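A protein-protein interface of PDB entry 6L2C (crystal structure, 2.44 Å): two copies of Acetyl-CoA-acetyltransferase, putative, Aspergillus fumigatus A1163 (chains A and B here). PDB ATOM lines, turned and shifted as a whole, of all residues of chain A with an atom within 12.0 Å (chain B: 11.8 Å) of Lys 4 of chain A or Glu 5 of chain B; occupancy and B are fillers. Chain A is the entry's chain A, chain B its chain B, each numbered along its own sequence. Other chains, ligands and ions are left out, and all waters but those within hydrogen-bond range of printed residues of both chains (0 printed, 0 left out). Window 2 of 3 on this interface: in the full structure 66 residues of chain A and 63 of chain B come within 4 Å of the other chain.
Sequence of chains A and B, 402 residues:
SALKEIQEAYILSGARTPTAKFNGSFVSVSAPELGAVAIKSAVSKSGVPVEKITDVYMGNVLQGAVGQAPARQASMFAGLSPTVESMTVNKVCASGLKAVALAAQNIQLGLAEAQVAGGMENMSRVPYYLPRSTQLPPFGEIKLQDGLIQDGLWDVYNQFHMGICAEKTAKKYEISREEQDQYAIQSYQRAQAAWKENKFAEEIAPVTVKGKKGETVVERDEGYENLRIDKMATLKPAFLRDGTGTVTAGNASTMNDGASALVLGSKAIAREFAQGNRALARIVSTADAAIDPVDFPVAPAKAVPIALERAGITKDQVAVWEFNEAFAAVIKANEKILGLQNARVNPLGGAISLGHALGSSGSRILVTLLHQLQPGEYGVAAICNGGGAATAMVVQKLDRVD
Hydrophobic or aromatic side chains of chain B within 4 Å of the printed part of chain A: Ile 6, Leu 109 and Leu 111.
Printed residues of chain A that touch a printed residue of chain B: Ser 1, Leu 3, Lys 4, Glu 5, Ile 6, Gln 105, Gln 108 and Leu 109.
Among the printed residues, 16 pairs touch across the chains.
Among the printed residues, Asp or Glu carboxylates within 4 Å of a Lys or Arg side-chain nitrogen of the other chain: Glu 5 of chain A with Lys 4 of chain B (3.9 Å).
NE2 of Gln 7 of chain A lies within hydrogen-bond range of O of Glu 5 of chain A.
The backbone carbonyl oxygen (O) of Asn 106 of chain B sits at hydrogen-bond distance from the backbone NH (N) of Leu 111 of chain B (2.9 Å).
N of Leu 3 of chain A sits at hydrogen-bond distance from O of Leu 109 of chain A, at 3.5 Å.
O of Asn 106 of chain B lies within hydrogen-bond range of N of Ala 112 of chain B, 3.4 Å away.
The backbone carbonyl oxygen (O) of Gln 108 of chain A lies within hydrogen-bond range of the backbone NH (N) of Gln 7 of chain A (2.8 Å).
Arg 310 of chain B touches Ser 1 of chain A.
CD1 of Ile 6 of chain B touches O of Leu 3 of chain A (2.8 Å).
O of Lys 4 of chain A touches CG of Glu 5 of chain B, 3.5 Å away.
Glu 5 of chain A touches Ile 6 of chain B (O to CD1, 3.8 Å).
Leu 109 of chain B touches Ile 6 of chain A.
Gln 105 of chain A touches Leu 111 of chain B.
NE2 of Gln 108 of chain A touches CD1 of Leu 109 of chain B, at 3.8 Å.
Leu 109 of chain A touches Ile 6 of chain B (O to CD1, 3.7 Å).
CD1 of Leu 109 of chain A touches CG of Gln 105 of chain B, 3.6 Å away.
Leu 109 of chain A touches Leu 109 of chain B (CD2 to CD2, 3.6 Å).
Lys 4 of chain A touches two residues of chain B.
Glu 5 of chain B touches just one residue of chain A: Lys 4 (3.5 Å).
No residue of chain B comes within 4 Å of Ala 2 of chain A.
Glu 5 of chain A touches two residues of chain B.
Ile 6 of chain A touches just these residues of chain B: Lys 4 (3.3 Å) and Leu 109 (3.8 Å).
Of chain A, only Glu 5 (3.7 Å) and Ile 6 (3.3 Å) come within 4 Å of Lys 4 of chain B.
No residue of chain A comes within 4 Å of Gln 7 of chain B.
Of the printed residues of chain B, Gln 105 of chain A touches Gln 105, Asn 106, Leu 109 and Leu 111.
Printed residues of chain B within 4 Å of Ser 1 of chain A: Arg 310.
Of the printed residues of chain A, Leu 109 of chain B touches Ile 6 (3.8 Å), Gln 105 (3.5 Å), Gln 108 (3.8 Å) and Leu 109 (3.6 Å).
Gly 110 of chain A touches none of the printed residues of chain B.
Glu 8 of chain B touches none of the printed residues of chain A.
Lys 4 of chain A touches Ile 6 of chain B, and with the chains exchanged Ile 6 of chain A touches Lys 4 of chain B.
Gln 105 of chain A touches Asn 106 of chain B, but with the chains exchanged Asn 106 of chain A does not touch Gln 105 of chain B (4.03 Å).
Gln 105 of chain A touches Leu 109 of chain B, and with the chains exchanged Leu 109 of chain A touches Gln 105 of chain B.
Gln 108 of chain A touches Leu 109 of chain B, but with the chains exchanged Leu 109 of chain A does not touch Gln 108 of chain B (4.1 Å).
Positions printed for both chains: 4, 5, 6, 7, 8, 105, 106, 107, 108, 109, 110, 111 and 112.
Of the 16 pairs that touch across the chains among the printed residues, 10 have their exchanged pair printed and touching as well.
N of Ile 6 of chain B lies within hydrogen-bond range of O of Lys 4 of chain A, 3.0 Å away.
The side-chain carboxylate (OE1) of Glu 5 of chain A is in salt-bridge range of the side-chain amino group (NZ) of Lys 4 of chain B (3.9 Å).
NE2 of Gln 105 of chain A sits at hydrogen-bond distance from OD1 of Asn 106 of chain B, 3.3 Å away.
The side-chain amide oxygen of Gln 105 of chain A sits at hydrogen-bond distance from the side-chain amide nitrogen of Gln 105 of chain B.
The backbone carbonyl oxygen (O) of Lys 4 of chain B is in hydrogen-bond range of the backbone NH (N) of Ile 6 of chain A (3.3 Å).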
ATOM      1  N   SER A   1     -32.934 -15.274 -15.518  1.00  0.00           N
ATOM      2  CA  SER A   1     -31.934 -16.000 -16.341  1.00  0.00           C
ATOM      3  C   SER A   1     -30.563 -16.023 -15.642  1.00  0.00           C
ATOM      4  O   SER A   1     -30.338 -16.997 -14.904  1.00  0.00           O
ATOM      5  CB  SER A   1     -31.868 -15.429 -17.734  1.00  0.00           C
ATOM      6  OG  SER A   1     -33.109 -14.856 -18.114  1.00  0.00           O
ATOM      7  N   ALA A   2     -29.734 -14.992 -15.909  1.00  0.00           N
ATOM      8  CA  ALA A   2     -28.351 -14.653 -15.450  1.00  0.00           C
ATOM      9  C   ALA A   2     -27.278 -15.228 -16.385  1.00  0.00           C
ATOM     10  O   ALA A   2     -27.663 -15.741 -17.442  1.00  0.00           O
ATOM     11  CB  ALA A   2     -28.084 -14.945 -13.993  1.00  0.00           C
ATOM     12  N   LEU A   3     -25.992 -15.080 -16.031  1.00  0.00           N
ATOM     13  CA  LEU A   3     -24.827 -15.605 -16.809  1.00  0.00           C
ATOM     14  C   LEU A   3     -23.557 -15.539 -15.958  1.00  0.00           C
ATOM     15  O   LEU A   3     -23.435 -14.608 -15.189  1.00  0.00           O
ATOM     16  CB  LEU A   3     -24.655 -14.853 -18.129  1.00  0.00           C
ATOM     17  CG  LEU A   3     -24.895 -15.729 -19.361  1.00  0.00           C
ATOM     18  CD1 LEU A   3     -25.697 -15.001 -20.433  1.00  0.00           C
ATOM     19  CD2 LEU A   3     -23.590 -16.260 -19.927  1.00  0.00           C
ATOM     20  N   LYS A   4     -22.640 -16.492 -16.121  1.00  0.00           N
ATOM     21  CA  LYS A   4     -21.428 -16.558 -15.264  1.00  0.00           C
ATOM     22  C   LYS A   4     -20.362 -15.574 -15.731  1.00  0.00           C
ATOM     23  O   LYS A   4     -19.562 -15.154 -14.908  1.00  0.00           O
ATOM     24  CB  LYS A   4     -20.810 -17.956 -15.312  1.00  0.00           C
ATOM     25  CG  LYS A   4     -21.561 -18.984 -16.143  1.00  0.00           C
ATOM     26  CD  LYS A   4     -21.349 -18.858 -17.635  1.00  0.00           C
ATOM     27  CE  LYS A   4     -22.613 -19.139 -18.413  1.00  0.00           C
ATOM     28  NZ  LYS A   4     -23.642 -19.770 -17.556  1.00  0.00           N
ATOM     29  N   GLU A   5     -20.347 -15.253 -17.017  1.00  0.00           N
ATOM     30  CA  GLU A   5     -19.307 -14.341 -17.542  1.00  0.00           C
ATOM     31  C   GLU A   5     -19.958 -13.055 -18.041  1.00  0.00           C
ATOM     32  O   GLU A   5     -21.083 -13.118 -18.516  1.00  0.00           O
ATOM     33  CB  GLU A   5     -18.512 -15.047 -18.643  1.00  0.00           C
ATOM     34  CG  GLU A   5     -19.292 -16.140 -19.361  1.00  0.00           C
ATOM     35  CD  GLU A   5     -18.785 -16.454 -20.761  1.00  0.00           C
ATOM     36  OE1 GLU A   5     -17.753 -17.132 -20.870  1.00  0.00           O
ATOM     37  OE2 GLU A   5     -19.415 -16.019 -21.735  1.00  0.00           O
ATOM     38  N   ILE A   6     -19.247 -11.942 -17.905  1.00  0.00           N
ATOM     39  CA  ILE A   6     -19.724 -10.608 -18.363  1.00  0.00           C
ATOM     40  C   ILE A   6     -19.854 -10.648 -19.882  1.00  0.00           C
ATOM     41  O   ILE A   6     -18.860 -10.911 -20.546  1.00  0.00           O
ATOM     42  CB  ILE A   6     -18.719  -9.525 -17.948  1.00  0.00           C
ATOM     43  CG1 ILE A   6     -18.639  -9.352 -16.435  1.00  0.00           C
ATOM     44  CG2 ILE A   6     -18.999  -8.219 -18.661  1.00  0.00           C
ATOM     45  CD1 ILE A   6     -17.374  -8.684 -15.988  1.00  0.00           C
ATOM     46  N   GLN A   7     -21.042 -10.372 -20.400  1.00  0.00           N
ATOM     47  CA  GLN A   7     -21.233 -10.392 -21.862  1.00  0.00           C
ATOM     48  C   GLN A   7     -20.897  -9.022 -22.448  1.00  0.00           C
ATOM     49  O   GLN A   7     -20.740  -8.071 -21.699  1.00  0.00           O
ATOM     50  CB  GLN A   7     -22.685 -10.710 -22.192  1.00  0.00           C
ATOM     51  CG  GLN A   7     -23.230 -11.904 -21.441  1.00  0.00           C
ATOM     52  CD  GLN A   7     -22.667 -13.191 -21.979  1.00  0.00           C
ATOM     53  OE1 GLN A   7     -23.133 -13.721 -22.977  1.00  0.00           O
ATOM     54  NE2 GLN A   7     -21.639 -13.689 -21.322  1.00  0.00           N
ATOM     55  N   GLU A   8     -20.721  -8.991 -23.760  1.00  0.00           N
ATOM     56  CA  GLU A   8     -20.531  -7.753 -24.537  1.00  0.00           C
ATOM     57  C   GLU A   8     -21.876  -7.124 -24.883  1.00  0.00           C
ATOM     58  O   GLU A   8     -22.857  -7.842 -25.115  1.00  0.00           O
ATOM     59  CB  GLU A   8     -19.838  -8.039 -25.876  1.00  0.00           C
ATOM     60  CG  GLU A   8     -18.447  -8.655 -25.810  1.00  0.00           C
ATOM     61  CD  GLU A   8     -17.389  -7.716 -25.261  1.00  0.00           C
ATOM     62  OE1 GLU A   8     -16.256  -8.209 -25.080  1.00  0.00           O
ATOM     63  OE2 GLU A   8     -17.675  -6.506 -25.010  1.00  0.00           O
ATOM     64  N   GLN A 105     -25.548  -2.700 -18.794  1.00  0.00           N
ATOM     65  CA  GLN A 105     -25.230  -3.621 -17.679  1.00  0.00           C
ATOM     66  C   GLN A 105     -26.203  -4.797 -17.686  1.00  0.00           C
ATOM     67  O   GLN A 105     -25.781  -5.895 -17.400  1.00  0.00           O
ATOM     68  CB  GLN A 105     -25.245  -2.883 -16.351  1.00  0.00           C
ATOM     69  CG  GLN A 105     -24.116  -1.897 -16.200  1.00  0.00           C
ATOM     70  CD  GLN A 105     -24.078  -1.370 -14.796  1.00  0.00           C
ATOM     71  OE1 GLN A 105     -25.012  -1.534 -14.028  1.00  0.00           O
ATOM     72  NE2 GLN A 105     -22.977  -0.749 -14.448  1.00  0.00           N
ATOM     73  N   ASN A 106     -27.458  -4.546 -18.035  1.00  0.00           N
ATOM     74  CA  ASN A 106     -28.478  -5.613 -18.148  1.00  0.00           C
ATOM     75  C   ASN A 106     -28.001  -6.660 -19.150  1.00  0.00           C
ATOM     76  O   ASN A 106     -28.132  -7.833 -18.873  1.00  0.00           O
ATOM     77  CB  ASN A 106     -29.809  -5.044 -18.609  1.00  0.00           C
ATOM     78  CG  ASN A 106     -30.495  -4.278 -17.510  1.00  0.00           C
ATOM     79  OD1 ASN A 106     -30.253  -4.527 -16.348  1.00  0.00           O
ATOM     80  ND2 ASN A 106     -31.333  -3.339 -17.874  1.00  0.00           N
ATOM     81  N   ILE A 107     -27.501  -6.211 -20.292  1.00  0.00           N
ATOM     82  CA  ILE A 107     -26.985  -7.116 -21.344  1.00  0.00           C
ATOM     83  C   ILE A 107     -25.673  -7.746 -20.867  1.00  0.00           C
ATOM     84  O   ILE A 107     -25.522  -8.942 -21.034  1.00  0.00           O
ATOM     85  CB  ILE A 107     -26.883  -6.340 -22.664  1.00  0.00           C
ATOM     86  CG1 ILE A 107     -28.278  -6.102 -23.230  1.00  0.00           C
ATOM     87  CG2 ILE A 107     -25.994  -7.049 -23.660  1.00  0.00           C
ATOM     88  CD1 ILE A 107     -28.317  -5.185 -24.402  1.00  0.00           C
ATOM     89  N   GLN A 108     -24.814  -6.975 -20.203  1.00  0.00           N
ATOM     90  CA  GLN A 108     -23.500  -7.448 -19.698  1.00  0.00           C
ATOM     91  C   GLN A 108     -23.671  -8.529 -18.635  1.00  0.00           C
ATOM     92  O   GLN A 108     -22.795  -9.357 -18.522  1.00  0.00           O
ATOM     93  CB  GLN A 108     -22.728  -6.294 -19.067  1.00  0.00           C
ATOM     94  CG  GLN A 108     -22.099  -5.354 -20.070  1.00  0.00           C
ATOM     95  CD  GLN A 108     -21.648  -4.058 -19.451  1.00  0.00           C
ATOM     96  OE1 GLN A 108     -21.933  -2.990 -19.950  1.00  0.00           O
ATOM     97  NE2 GLN A 108     -20.923  -4.132 -18.358  1.00  0.00           N
ATOM     98  N   LEU A 109     -24.745  -8.472 -17.858  1.00  0.00           N
ATOM     99  CA  LEU A 109     -25.004  -9.458 -16.792  1.00  0.00           C
ATOM    100  C   LEU A 109     -25.761 -10.644 -17.384  1.00  0.00           C
ATOM    101  O   LEU A 109     -25.788 -11.678 -16.746  1.00  0.00           O
ATOM    102  CB  LEU A 109     -25.809  -8.771 -15.693  1.00  0.00           C
ATOM    103  CG  LEU A 109     -25.017  -7.832 -14.793  1.00  0.00           C
ATOM    104  CD1 LEU A 109     -25.936  -6.903 -14.047  1.00  0.00           C
ATOM    105  CD2 LEU A 109     -24.188  -8.608 -13.810  1.00  0.00           C
ATOM    106  N   GLY A 110     -26.333 -10.485 -18.574  1.00  0.00           N
ATOM    107  CA  GLY A 110     -27.067 -11.582 -19.216  1.00  0.00           C
ATOM    108  C   GLY A 110     -28.511 -11.596 -18.798  1.00  0.00           C
ATOM    109  O   GLY A 110     -29.144 -12.610 -18.978  1.00  0.00           O
ATOM    110  N   LEU A 111     -29.009 -10.480 -18.281  1.00  0.00           N
ATOM    111  CA  LEU A 111     -30.416 -10.393 -17.828  1.00  0.00           C
ATOM    112  C   LEU A 111     -31.301  -9.939 -18.977  1.00  0.00           C
ATOM    113  O   LEU A 111     -32.501 -10.106 -18.877  1.00  0.00           O
ATOM    114  CB  LEU A 111     -30.515  -9.379 -16.693  1.00  0.00           C
ATOM    115  CG  LEU A 111     -29.521  -9.547 -15.556  1.00  0.00           C
ATOM    116  CD1 LEU A 111     -29.751  -8.478 -14.515  1.00  0.00           C
ATOM    117  CD2 LEU A 111     -29.629 -10.927 -14.943  1.00  0.00           C
ATOM    118  N   ALA A 112     -30.716  -9.369 -20.016  1.00  0.00           N
ATOM    119  CA  ALA A 112     -31.547  -8.890 -21.132  1.00  0.00           C
ATOM    120  C   ALA A 112     -30.787  -9.042 -22.440  1.00  0.00           C
ATOM    121  O   ALA A 112     -29.584  -9.188 -22.389  1.00  0.00           O
ATOM    122  CB  ALA A 112     -31.929  -7.464 -20.888  1.00  0.00           C
ATOM    123  N   LYS B   4     -13.897 -10.311 -14.870  1.00  0.00           N
ATOM    124  CA  LYS B   4     -14.464 -10.910 -16.107  1.00  0.00           C
ATOM    125  C   LYS B   4     -15.490 -11.982 -15.739  1.00  0.00           C
ATOM    126  O   LYS B   4     -16.231 -12.430 -16.609  1.00  0.00           O
ATOM    127  CB  LYS B   4     -13.349 -11.465 -16.992  1.00  0.00           C
ATOM    128  CG  LYS B   4     -13.448 -12.953 -17.294  1.00  0.00           C
ATOM    129  CD  LYS B   4     -13.680 -13.265 -18.747  1.00  0.00           C
ATOM    130  CE  LYS B   4     -13.310 -14.687 -19.103  1.00  0.00           C
ATOM    131  NZ  LYS B   4     -14.500 -15.502 -19.438  1.00  0.00           N
ATOM    132  N   GLU B   5     -15.495 -12.400 -14.477  1.00  0.00           N
ATOM    133  CA  GLU B   5     -16.489 -13.386 -13.979  1.00  0.00           C
ATOM    134  C   GLU B   5     -17.453 -12.635 -13.058  1.00  0.00           C
ATOM    135  O   GLU B   5     -16.978 -11.867 -12.233  1.00  0.00           O
ATOM    136  CB  GLU B   5     -15.784 -14.523 -13.237  1.00  0.00           C
ATOM    137  CG  GLU B   5     -16.425 -15.883 -13.464  1.00  0.00           C
ATOM    138  CD  GLU B   5     -15.543 -16.895 -14.179  1.00  0.00           C
ATOM    139  OE1 GLU B   5     -15.294 -17.969 -13.602  1.00  0.00           O
ATOM    140  OE2 GLU B   5     -15.095 -16.603 -15.302  1.00  0.00           O
ATOM    141  N   ILE B   6     -18.754 -12.847 -13.210  1.00  0.00           N
ATOM    142  CA  ILE B   6     -19.731 -12.102 -12.381  1.00  0.00           C
ATOM    143  C   ILE B   6     -19.634 -12.531 -10.922  1.00  0.00           C
ATOM    144  O   ILE B   6     -19.638 -13.717 -10.675  1.00  0.00           O
ATOM    145  CB  ILE B   6     -21.133 -12.287 -12.963  1.00  0.00           C
ATOM    146  CG1 ILE B   6     -21.214 -11.647 -14.347  1.00  0.00           C
ATOM    147  CG2 ILE B   6     -22.176 -11.739 -12.016  1.00  0.00           C
ATOM    148  CD1 ILE B   6     -22.458 -12.000 -15.105  1.00  0.00           C
ATOM    149  N   GLN B   7     -19.590 -11.586  -9.992  1.00  0.00           N
ATOM    150  CA  GLN B   7     -19.505 -11.951  -8.566  1.00  0.00           C
ATOM    151  C   GLN B   7     -20.824 -11.677  -7.858  1.00  0.00           C
ATOM    152  O   GLN B   7     -21.790 -11.302  -8.505  1.00  0.00           O
ATOM    153  CB  GLN B   7     -18.501 -11.078  -7.834  1.00  0.00           C
ATOM    154  CG  GLN B   7     -17.472 -10.427  -8.722  1.00  0.00           C
ATOM    155  CD  GLN B   7     -16.186 -10.392  -7.948  1.00  0.00           C
ATOM    156  OE1 GLN B   7     -16.032  -9.630  -6.999  1.00  0.00           O
ATOM    157  NE2 GLN B   7     -15.270 -11.268  -8.328  1.00  0.00           N
ATOM    158  N   GLU B   8     -20.799 -11.848  -6.544  1.00  0.00           N
ATOM    159  CA  GLU B   8     -21.983 -11.626  -5.695  1.00  0.00           C
ATOM    160  C   GLU B   8     -21.821 -10.315  -4.934  1.00  0.00           C
ATOM    161  O   GLU B   8     -20.708  -9.845  -4.804  1.00  0.00           O
ATOM    162  CB  GLU B   8     -22.114 -12.757  -4.688  1.00  0.00           C
ATOM    163  CG  GLU B   8     -21.956 -14.136  -5.279  1.00  0.00           C
ATOM    164  CD  GLU B   8     -21.711 -15.182  -4.210  1.00  0.00           C
ATOM    165  OE1 GLU B   8     -20.670 -15.111  -3.541  1.00  0.00           O
ATOM    166  OE2 GLU B   8     -22.571 -16.043  -4.038  1.00  0.00           O
ATOM    167  N   ALA B   9     -22.935  -9.759  -4.483  1.00  0.00           N
ATOM    168  CA  ALA B   9     -22.940  -8.511  -3.702  1.00  0.00           C
ATOM    169  C   ALA B   9     -23.526  -8.833  -2.335  1.00  0.00           C
ATOM    170  O   ALA B   9     -24.402  -9.664  -2.256  1.00  0.00           O
ATOM    171  CB  ALA B   9     -23.740  -7.463  -4.414  1.00  0.00           C
ATOM    172  N   ALA B 104     -25.811  -2.961  -6.495  1.00  0.00           N
ATOM    173  CA  ALA B 104     -25.401  -4.355  -6.496  1.00  0.00           C
ATOM    174  C   ALA B 104     -24.767  -4.716  -7.871  1.00  0.00           C
ATOM    175  O   ALA B 104     -23.747  -5.419  -7.934  1.00  0.00           O
ATOM    176  CB  ALA B 104     -26.580  -5.273  -6.165  1.00  0.00           C
ATOM    177  N   GLN B 105     -25.346  -4.212  -8.959  1.00  0.00           N
ATOM    178  CA  GLN B 105     -24.802  -4.502 -10.287  1.00  0.00           C
ATOM    179  C   GLN B 105     -23.359  -4.068 -10.434  1.00  0.00           C
ATOM    180  O   GLN B 105     -22.580  -4.800 -11.008  1.00  0.00           O
ATOM    181  CB  GLN B 105     -25.675  -3.927 -11.386  1.00  0.00           C
ATOM    182  CG  GLN B 105     -27.001  -4.665 -11.493  1.00  0.00           C
ATOM    183  CD  GLN B 105     -27.917  -4.132 -12.552  1.00  0.00           C
ATOM    184  OE1 GLN B 105     -29.108  -4.379 -12.491  1.00  0.00           O
ATOM    185  NE2 GLN B 105     -27.380  -3.377 -13.528  1.00  0.00           N
ATOM    186  N   ASN B 106     -22.982  -2.914  -9.876  1.00  0.00           N
ATOM    187  CA  ASN B 106     -21.578  -2.470  -9.927  1.00  0.00           C
ATOM    188  C   ASN B 106     -20.662  -3.483  -9.263  1.00  0.00           C
ATOM    189  O   ASN B 106     -19.578  -3.771  -9.776  1.00  0.00           O
ATOM    190  CB  ASN B 106     -21.359  -1.084  -9.292  1.00  0.00           C
ATOM    191  CG  ASN B 106     -21.927   0.055 -10.127  1.00  0.00           C
ATOM    192  OD1 ASN B 106     -22.157  -0.080 -11.320  1.00  0.00           O
ATOM    193  ND2 ASN B 106     -22.129   1.193  -9.503  1.00  0.00           N
ATOM    194  N   ILE B 107     -21.092  -4.023  -8.127  1.00  0.00           N
ATOM    195  CA  ILE B 107     -20.257  -4.957  -7.394  1.00  0.00           C
ATOM    196  C   ILE B 107     -20.192  -6.271  -8.167  1.00  0.00           C
ATOM    197  O   ILE B 107     -19.139  -6.899  -8.234  1.00  0.00           O
ATOM    198  CB  ILE B 107     -20.782  -5.161  -5.971  1.00  0.00           C
ATOM    199  CG1 ILE B 107     -20.510  -3.900  -5.163  1.00  0.00           C
ATOM    200  CG2 ILE B 107     -20.115  -6.357  -5.308  1.00  0.00           C
ATOM    201  CD1 ILE B 107     -21.225  -3.838  -3.821  1.00  0.00           C
ATOM    202  N   GLN B 108     -21.320  -6.659  -8.752  1.00  0.00           N
ATOM    203  CA  GLN B 108     -21.419  -7.860  -9.550  1.00  0.00           C
ATOM    204  C   GLN B 108     -20.503  -7.840 -10.805  1.00  0.00           C
ATOM    205  O   GLN B 108     -19.843  -8.832 -11.123  1.00  0.00           O
ATOM    206  CB  GLN B 108     -22.887  -8.128  -9.940  1.00  0.00           C
ATOM    207  CG  GLN B 108     -23.778  -8.524  -8.752  1.00  0.00           C
ATOM    208  CD  GLN B 108     -25.290  -8.387  -8.997  1.00  0.00           C
ATOM    209  OE1 GLN B 108     -25.746  -8.093 -10.083  1.00  0.00           O
ATOM    210  NE2 GLN B 108     -26.064  -8.627  -7.968  1.00  0.00           N
ATOM    211  N   LEU B 109     -20.459  -6.719 -11.502  1.00  0.00           N
ATOM    212  CA  LEU B 109     -19.613  -6.568 -12.689  1.00  0.00           C
ATOM    213  C   LEU B 109     -18.157  -6.233 -12.339  1.00  0.00           C
ATOM    214  O   LEU B 109     -17.340  -6.033 -13.235  1.00  0.00           O
ATOM    215  CB  LEU B 109     -20.183  -5.464 -13.584  1.00  0.00           C
ATOM    216  CG  LEU B 109     -21.556  -5.720 -14.195  1.00  0.00           C
ATOM    217  CD1 LEU B 109     -22.095  -4.425 -14.788  1.00  0.00           C
ATOM    218  CD2 LEU B 109     -21.462  -6.801 -15.268  1.00  0.00           C
ATOM    219  N   GLY B 110     -17.839  -6.134 -11.059  1.00  0.00           N
ATOM    220  CA  GLY B 110     -16.481  -5.890 -10.627  1.00  0.00           C
ATOM    221  C   GLY B 110     -15.991  -4.461 -10.754  1.00  0.00           C
ATOM    222  O   GLY B 110     -14.832  -4.196 -10.527  1.00  0.00           O
ATOM    223  N   LEU B 111     -16.902  -3.529 -10.985  1.00  0.00           N
ATOM    224  CA  LEU B 111     -16.512  -2.103 -11.085  1.00  0.00           C
ATOM    225  C   LEU B 111     -16.346  -1.481  -9.696  1.00  0.00           C
ATOM    226  O   LEU B 111     -15.789  -0.405  -9.633  1.00  0.00           O
ATOM    227  CB  LEU B 111     -17.561  -1.330 -11.881  1.00  0.00           C
ATOM    228  CG  LEU B 111     -18.004  -1.946 -13.196  1.00  0.00           C
ATOM    229  CD1 LEU B 111     -19.430  -1.552 -13.495  1.00  0.00           C
ATOM    230  CD2 LEU B 111     -17.106  -1.499 -14.324  1.00  0.00           C
ATOM    231  N   ALA B 112     -16.798  -2.123  -8.627  1.00  0.00           N
ATOM    232  CA  ALA B 112     -16.647  -1.496  -7.297  1.00  0.00           C
ATOM    233  C   ALA B 112     -16.645  -2.537  -6.181  1.00  0.00           C
ATOM    234  O   ALA B 112     -17.175  -3.608  -6.373  1.00  0.00           O
ATOM    235  CB  ALA B 112     -17.747  -0.501  -7.084  1.00  0.00           C
ATOM    236  N   SER B 266     -18.465  -6.333  -1.777  1.00  0.00           N
ATOM    237  CA  SER B 266     -18.000  -7.596  -2.419  1.00  0.00           C
ATOM    238  C   SER B 266     -17.780  -8.644  -1.352  1.00  0.00           C
ATOM    239  O   SER B 266     -17.702  -8.318  -0.181  1.00  0.00           O
ATOM    240  CB  SER B 266     -16.691  -7.383  -3.138  1.00  0.00           C
ATOM    241  OG  SER B 266     -15.731  -7.010  -2.150  1.00  0.00           O
ATOM    242  N   LYS B 267     -17.669  -9.899  -1.763  1.00  0.00           N
ATOM    243  CA  LYS B 267     -17.324 -11.001  -0.836  1.00  0.00           C
ATOM    244  C   LYS B 267     -16.083 -10.687   0.010  1.00  0.00           C
ATOM    245  O   LYS B 267     -16.067 -10.869   1.227  1.00  0.00           O
ATOM    246  CB  LYS B 267     -17.103 -12.282  -1.624  1.00  0.00           C
ATOM    247  CG  LYS B 267     -16.766 -13.488  -0.773  1.00  0.00           C
ATOM    248  CD  LYS B 267     -17.247 -14.794  -1.400  1.00  0.00           C
ATOM    249  CE  LYS B 267     -16.601 -15.979  -0.686  1.00  0.00           C
ATOM    250  NZ  LYS B 267     -17.513 -17.124  -0.427  1.00  0.00           N
ATOM    251  N   ARG B 310     -34.375 -17.024 -10.210  1.00  0.00           N
ATOM    252  CA  ARG B 310     -32.939 -16.665 -10.319  1.00  0.00           C
ATOM    253  C   ARG B 310     -32.188 -16.948  -9.021  1.00  0.00           C
ATOM    254  O   ARG B 310     -30.975 -17.041  -9.083  1.00  0.00           O
ATOM    255  CB  ARG B 310     -32.764 -15.207 -10.729  1.00  0.00           C
ATOM    256  CG  ARG B 310     -33.755 -14.731 -11.775  1.00  0.00           C
ATOM    257  CD  ARG B 310     -33.101 -13.951 -12.892  1.00  0.00           C
ATOM    258  NE  ARG B 310     -33.106 -12.527 -12.654  1.00  0.00           N
ATOM    259  CZ  ARG B 310     -33.657 -11.631 -13.448  1.00  0.00           C
ATOM    260  NH1 ARG B 310     -34.262 -12.003 -14.553  1.00  0.00           N
ATOM    261  NH2 ARG B 310     -33.604 -10.359 -13.134  1.00  0.00           N
